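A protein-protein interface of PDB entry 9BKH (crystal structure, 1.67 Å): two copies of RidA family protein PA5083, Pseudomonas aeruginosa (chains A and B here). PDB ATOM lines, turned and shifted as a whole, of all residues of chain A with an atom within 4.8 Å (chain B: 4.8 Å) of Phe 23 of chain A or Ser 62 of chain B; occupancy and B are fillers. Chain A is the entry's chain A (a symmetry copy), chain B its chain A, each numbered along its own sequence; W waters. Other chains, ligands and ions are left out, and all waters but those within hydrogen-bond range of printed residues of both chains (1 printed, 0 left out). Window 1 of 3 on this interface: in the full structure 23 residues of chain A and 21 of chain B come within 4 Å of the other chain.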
ATOM      1  N   ALA A  14       5.002  -9.831 -27.174  1.00  0.00           N
ATOM      2  CA  ALA A  14       4.125 -10.886 -27.662  1.00  0.00           C
ATOM      3  C   ALA A  14       4.926 -12.051 -28.220  1.00  0.00           C
ATOM      4  O   ALA A  14       4.512 -13.203 -28.088  1.00  0.00           O
ATOM      5  CB  ALA A  14       3.166 -10.340 -28.726  1.00  0.00           C
ATOM      6  N   ALA A  15       6.055 -11.767 -28.893  1.00  0.00           N
ATOM      7  CA  ALA A  15       6.945 -12.794 -29.394  1.00  0.00           C
ATOM      8  C   ALA A  15       8.378 -12.311 -29.241  1.00  0.00           C
ATOM      9  O   ALA A  15       8.655 -11.117 -29.372  1.00  0.00           O
ATOM     10  CB  ALA A  15       6.686 -13.133 -30.860  1.00  0.00           C
ATOM     11  N   VAL A  16       9.260 -13.240 -28.902  1.00  0.00           N
ATOM     12  CA  VAL A  16      10.704 -13.032 -28.939  1.00  0.00           C
ATOM     13  C   VAL A  16      11.297 -14.088 -29.855  1.00  0.00           C
ATOM     14  O   VAL A  16      11.041 -15.288 -29.687  1.00  0.00           O
ATOM     15  CB  VAL A  16      11.334 -13.098 -27.537  1.00  0.00           C
ATOM     16  CG1 VAL A  16      12.840 -12.955 -27.640  1.00  0.00           C
ATOM     17  CG2 VAL A  16      10.773 -12.022 -26.639  1.00  0.00           C
ATOM     18  N   LEU A  21      14.313 -20.011 -33.336  1.00  0.00           N
ATOM     19  CA  LEU A  21      13.237 -20.258 -32.384  1.00  0.00           C
ATOM     20  C   LEU A  21      12.388 -19.010 -32.191  1.00  0.00           C
ATOM     21  O   LEU A  21      12.875 -17.880 -32.270  1.00  0.00           O
ATOM     22  CB  LEU A  21      13.784 -20.707 -31.027  1.00  0.00           C
ATOM     23  CG  LEU A  21      14.475 -22.068 -31.023  1.00  0.00           C
ATOM     24  CD1 LEU A  21      15.030 -22.302 -29.605  1.00  0.00           C
ATOM     25  CD2 LEU A  21      13.552 -23.179 -31.422  1.00  0.00           C
ATOM     26  N   VAL A  22      11.106 -19.244 -31.914  1.00  0.00           N
ATOM     27  CA  VAL A  22      10.111 -18.210 -31.672  1.00  0.00           C
ATOM     28  C   VAL A  22       9.431 -18.562 -30.357  1.00  0.00           C
ATOM     29  O   VAL A  22       8.873 -19.659 -30.232  1.00  0.00           O
ATOM     30  CB  VAL A  22       9.066 -18.129 -32.800  1.00  0.00           C
ATOM     31  CG1 VAL A  22       8.014 -17.143 -32.437  1.00  0.00           C
ATOM     32  CG2 VAL A  22       9.764 -17.801 -34.124  1.00  0.00           C
ATOM     33  N   PHE A  23       9.503 -17.652 -29.389  1.00  0.00           N
ATOM     34  CA  PHE A  23       8.862 -17.794 -28.083  1.00  0.00           C
ATOM     35  C   PHE A  23       7.694 -16.821 -27.996  1.00  0.00           C
ATOM     36  O   PHE A  23       7.891 -15.605 -28.010  1.00  0.00           O
ATOM     37  CB  PHE A  23       9.855 -17.507 -26.943  1.00  0.00           C
ATOM     38  CG  PHE A  23      11.025 -18.430 -26.923  1.00  0.00           C
ATOM     39  CD1 PHE A  23      12.087 -18.254 -27.810  1.00  0.00           C
ATOM     40  CD2 PHE A  23      11.081 -19.477 -26.019  1.00  0.00           C
ATOM     41  CE1 PHE A  23      13.186 -19.140 -27.794  1.00  0.00           C
ATOM     42  CE2 PHE A  23      12.168 -20.357 -26.003  1.00  0.00           C
ATOM     43  CZ  PHE A  23      13.224 -20.178 -26.894  1.00  0.00           C
ATOM     44  N   LEU A  24       6.480 -17.349 -27.876  1.00  0.00           N
ATOM     45  CA  LEU A  24       5.305 -16.496 -27.753  1.00  0.00           C
ATOM     46  C   LEU A  24       4.881 -16.347 -26.302  1.00  0.00           C
ATOM     47  O   LEU A  24       4.921 -17.312 -25.528  1.00  0.00           O
ATOM     48  CB  LEU A  24       4.144 -17.061 -28.552  1.00  0.00           C
ATOM     49  CG  LEU A  24       4.362 -17.240 -30.052  1.00  0.00           C
ATOM     50  CD1 LEU A  24       2.996 -17.585 -30.661  1.00  0.00           C
ATOM     51  CD2 LEU A  24       4.972 -16.026 -30.665  1.00  0.00           C
ATOM     52  N   SER A  25       4.443 -15.141 -25.945  1.00  0.00           N
ATOM     53  CA  SER A  25       3.751 -14.962 -24.675  1.00  0.00           C
ATOM     54  C   SER A  25       2.468 -15.785 -24.649  1.00  0.00           C
ATOM     55  O   SER A  25       1.812 -16.002 -25.672  1.00  0.00           O
ATOM     56  CB  SER A  25       3.423 -13.493 -24.438  1.00  0.00           C
ATOM     57  OG  SER A  25       4.579 -12.730 -24.143  1.00  0.00           O
ATOM     58  N   VAL A 111       3.067 -20.891 -26.698  1.00  0.00           N
ATOM     59  CA  VAL A 111       3.653 -21.643 -27.798  1.00  0.00           C
ATOM     60  C   VAL A 111       5.115 -21.271 -28.013  1.00  0.00           C
ATOM     61  O   VAL A 111       5.507 -20.107 -27.887  1.00  0.00           O
ATOM     62  CB  VAL A 111       2.819 -21.420 -29.084  1.00  0.00           C
ATOM     63  CG1 VAL A 111       3.677 -21.580 -30.326  1.00  0.00           C
ATOM     64  CG2 VAL A 111       1.609 -22.370 -29.096  1.00  0.00           C
ATOM     65  N   VAL A 112       5.915 -22.285 -28.322  1.00  0.00           N
ATOM     66  CA  VAL A 112       7.272 -22.150 -28.853  1.00  0.00           C
ATOM     67  C   VAL A 112       7.274 -22.812 -30.220  1.00  0.00           C
ATOM     68  O   VAL A 112       6.705 -23.901 -30.396  1.00  0.00           O
ATOM     69  CB  VAL A 112       8.321 -22.786 -27.929  1.00  0.00           C
ATOM     70  CG1 VAL A 112       9.736 -22.607 -28.535  1.00  0.00           C
ATOM     71  CG2 VAL A 112       8.281 -22.143 -26.582  1.00  0.00           C
ATOM     72  N   ILE B  60      16.790 -12.383 -21.995  1.00  0.00           N
ATOM     73  CA  ILE B  60      15.748 -13.331 -21.605  1.00  0.00           C
ATOM     74  C   ILE B  60      14.840 -13.578 -22.804  1.00  0.00           C
ATOM     75  O   ILE B  60      14.431 -12.635 -23.507  1.00  0.00           O
ATOM     76  CB  ILE B  60      14.966 -12.807 -20.395  1.00  0.00           C
ATOM     77  CG1 ILE B  60      15.883 -12.645 -19.183  1.00  0.00           C
ATOM     78  CG2 ILE B  60      13.830 -13.780 -20.052  1.00  0.00           C
ATOM     79  CD1 ILE B  60      15.245 -11.866 -18.033  1.00  0.00           C
ATOM     80  N   LEU B  61      14.505 -14.845 -23.038  1.00  0.00           N
ATOM     81  CA  LEU B  61      13.632 -15.240 -24.132  1.00  0.00           C
ATOM     82  C   LEU B  61      12.205 -15.487 -23.665  1.00  0.00           C
ATOM     83  O   LEU B  61      11.244 -15.044 -24.319  1.00  0.00           O
ATOM     84  CB  LEU B  61      14.191 -16.491 -24.817  1.00  0.00           C
ATOM     85  CG  LEU B  61      15.607 -16.329 -25.400  1.00  0.00           C
ATOM     86  CD1 LEU B  61      16.075 -17.657 -25.936  1.00  0.00           C
ATOM     87  CD2 LEU B  61      15.654 -15.269 -26.462  1.00  0.00           C
ATOM     88  N   SER B  62      12.054 -16.139 -22.515  1.00  0.00           N
ATOM     89  CA  SER B  62      10.735 -16.459 -21.977  1.00  0.00           C
ATOM     90  C   SER B  62      10.806 -16.516 -20.468  1.00  0.00           C
ATOM     91  O   SER B  62      11.818 -16.906 -19.887  1.00  0.00           O
ATOM     92  CB  SER B  62      10.243 -17.797 -22.531  1.00  0.00           C
ATOM     93  OG  SER B  62      11.084 -18.843 -22.076  1.00  0.00           O
ATOM     94  N   ALA B  63       9.696 -16.157 -19.842  1.00  0.00           N
ATOM     95  CA  ALA B  63       9.502 -16.298 -18.414  1.00  0.00           C
ATOM     96  C   ALA B  63       8.095 -16.834 -18.181  1.00  0.00           C
ATOM     97  O   ALA B  63       7.136 -16.301 -18.739  1.00  0.00           O
ATOM     98  CB  ALA B  63       9.657 -14.958 -17.690  1.00  0.00           C
ATOM     99  N   THR B  64       7.977 -17.903 -17.412  1.00  0.00           N
ATOM    100  CA  THR B  64       6.693 -18.329 -16.857  1.00  0.00           C
ATOM    101  C   THR B  64       6.693 -17.947 -15.385  1.00  0.00           C
ATOM    102  O   THR B  64       7.601 -18.337 -14.636  1.00  0.00           O
ATOM    103  CB  THR B  64       6.419 -19.825 -17.047  1.00  0.00           C
ATOM    104  OG1 THR B  64       6.331 -20.109 -18.461  1.00  0.00           O
ATOM    105  CG2 THR B  64       5.084 -20.190 -16.380  1.00  0.00           C
ATOM    106  N   PRO B  91      10.746  -9.741 -22.114  1.00  0.00           N
ATOM    107  CA  PRO B  91      10.722 -11.039 -22.799  1.00  0.00           C
ATOM    108  C   PRO B  91       9.310 -11.520 -23.096  1.00  0.00           C
ATOM    109  O   PRO B  91       8.338 -10.864 -22.718  1.00  0.00           O
ATOM    110  CB  PRO B  91      11.421 -11.960 -21.777  1.00  0.00           C
ATOM    111  CG  PRO B  91      10.934 -11.406 -20.447  1.00  0.00           C
ATOM    112  CD  PRO B  91      10.876  -9.884 -20.653  1.00  0.00           C
ATOM    113  N   SER B  92       9.160 -12.672 -23.741  1.00  0.00           N
ATOM    114  CA  SER B  92       7.854 -13.321 -23.723  1.00  0.00           C
ATOM    115  C   SER B  92       7.550 -13.775 -22.296  1.00  0.00           C
ATOM    116  O   SER B  92       8.446 -14.107 -21.518  1.00  0.00           O
ATOM    117  CB  SER B  92       7.790 -14.486 -24.715  1.00  0.00           C
ATOM    118  OG  SER B  92       8.518 -15.618 -24.312  1.00  0.00           O
ATOM    119  N   THR B 110      10.290 -19.036 -13.803  1.00  0.00           N
ATOM    120  CA  THR B 110      11.163 -19.899 -14.593  1.00  0.00           C
ATOM    121  C   THR B 110      11.545 -19.208 -15.890  1.00  0.00           C
ATOM    122  O   THR B 110      10.672 -18.852 -16.691  1.00  0.00           O
ATOM    123  CB  THR B 110      10.463 -21.222 -14.896  1.00  0.00           C
ATOM    124  OG1 THR B 110      10.049 -21.808 -13.659  1.00  0.00           O
ATOM    125  CG2 THR B 110      11.349 -22.124 -15.678  1.00  0.00           C
ATOM    126  N   VAL B 111      12.851 -19.067 -16.120  1.00  0.00           N
ATOM    127  CA  VAL B 111      13.367 -18.299 -17.244  1.00  0.00           C
ATOM    128  C   VAL B 111      14.197 -19.169 -18.181  1.00  0.00           C
ATOM    129  O   VAL B 111      14.939 -20.054 -17.748  1.00  0.00           O
ATOM    130  CB  VAL B 111      14.186 -17.095 -16.719  1.00  0.00           C
ATOM    131  CG1 VAL B 111      15.253 -16.683 -17.718  1.00  0.00           C
ATOM    132  CG2 VAL B 111      13.244 -15.930 -16.372  1.00  0.00           C
ATOM    133  N   VAL B 112      14.040 -18.911 -19.475  1.00  0.00           N
ATOM    134  CA  VAL B 112      14.922 -19.396 -20.537  1.00  0.00           C
ATOM    135  C   VAL B 112      15.510 -18.168 -21.210  1.00  0.00           C
ATOM    136  O   VAL B 112      14.796 -17.188 -21.473  1.00  0.00           O
ATOM    137  CB  VAL B 112      14.177 -20.278 -21.549  1.00  0.00           C
ATOM    138  CG1 VAL B 112      15.157 -20.767 -22.646  1.00  0.00           C
ATOM    139  CG2 VAL B 112      13.580 -21.462 -20.864  1.00  0.00           C
HETATM  140  O   HOH W   1       7.068 -17.935 -24.028  1.00  0.00           O
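O of Val 112 of chain B lies within hydrogen-bond range of N of Leu 61 of chain B (2.8 Å).
The backbone carbonyl oxygen (O) of Ser 62 of chain B lies within hydrogen-bond range of the backbone NH (N) of Val 112 of chain B.
The side-chain hydroxyl (OG) of Ser 92 of chain B is in hydrogen-bond range of the backbone carbonyl oxygen (O) of Leu 61 of chain B.
The backbone NH (N) of Leu 24 of chain A is in hydrogen-bond range of the backbone carbonyl oxygen (O) of Val 111 of chain A.
The backbone NH (N) of Ala 63 of chain B lies within hydrogen-bond range of the backbone carbonyl oxygen (O) of Ser 92 of chain B (2.9 Å).
N of Ser 25 of chain A sits at hydrogen-bond distance from O of Ala 14 of chain A, 2.9 Å away.
CB of Val 16 of chain A touches O of Leu 61 of chain B (3.8 Å).
Val 16 of chain A touches Pro 91 of chain B.
CG2 of Val 16 of chain A touches N of Ser 92 of chain B (3.4 Å).
Leu 61 of chain B touches Phe 23 of chain A (CD1 to CE1, 3.7 Å).
CB of Ser 62 of chain B touches CD2 of Phe 23 of chain A, 3.96 Å away.
Phe 23 of chain A touches Ser 92 of chain B (O to CB, 3.5 Å).
Ser 92 of chain B touches Leu 24 of chain A (CB to C, 3.8 Å).
OG of Ser 25 of chain A touches CA of Ser 92 of chain B, 3.4 Å away.
Water W1 lies within hydrogen-bond range of the backbone carbonyl oxygen (O) of Leu 24 of chain A (2.7 Å) and the side-chain hydroxyl (OG) of Ser 92 of chain B (2.7 Å).
Ala 14 of chain A touches none of the printed residues of chain B.
Of the printed residues of chain B, Val 16 of chain A touches Leu 61, Pro 91 and Ser 92.
Of chain B, only Leu 61 (3.7 Å), Ser 62 (3.96 Å) and Ser 92 (3.5 Å) come within 4 Å of Phe 23 of chain A.
Of the printed residues of chain B, Leu 24 of chain A touches Ser 92 (3.8 Å).
Of the printed residues of chain B, Ser 25 of chain A touches Ser 92 (3.4 Å).
Of the printed residues of chain A, Leu 61 of chain B touches Val 16 and Phe 23.
Ser 62 of chain B touches one residue of chain A.
Of the printed residues of chain A, Pro 91 of chain B touches Val 16 (3.9 Å).
The nearest printed residue of chain A that does not touch Ser 62 of chain B is Val 16 of chain A (5.9 Å).
The nearest printed residue of chain A that does not touch Pro 91 of chain B is Ser 25 of chain A (4.4 Å).
Hydrophobic or aromatic side chains of chain A within 4 Å of the printed part of chain B: Val 16 and Phe 23.
Of the 10 printed residues of chain B, 4 touch a printed residue of chain A.
Hydrophobic or aromatic side chains of chain B that line the printed part of chain A: Leu 61.
Among the printed residues, no Asp or Glu carboxylate lies within 4 Å of a Lys or Arg side-chain nitrogen of the other chain.
2 positions are printed for both chains.
Of the 8 pairs that touch across the chains among the printed residues, none has its exchanged pair printed and touching as well.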
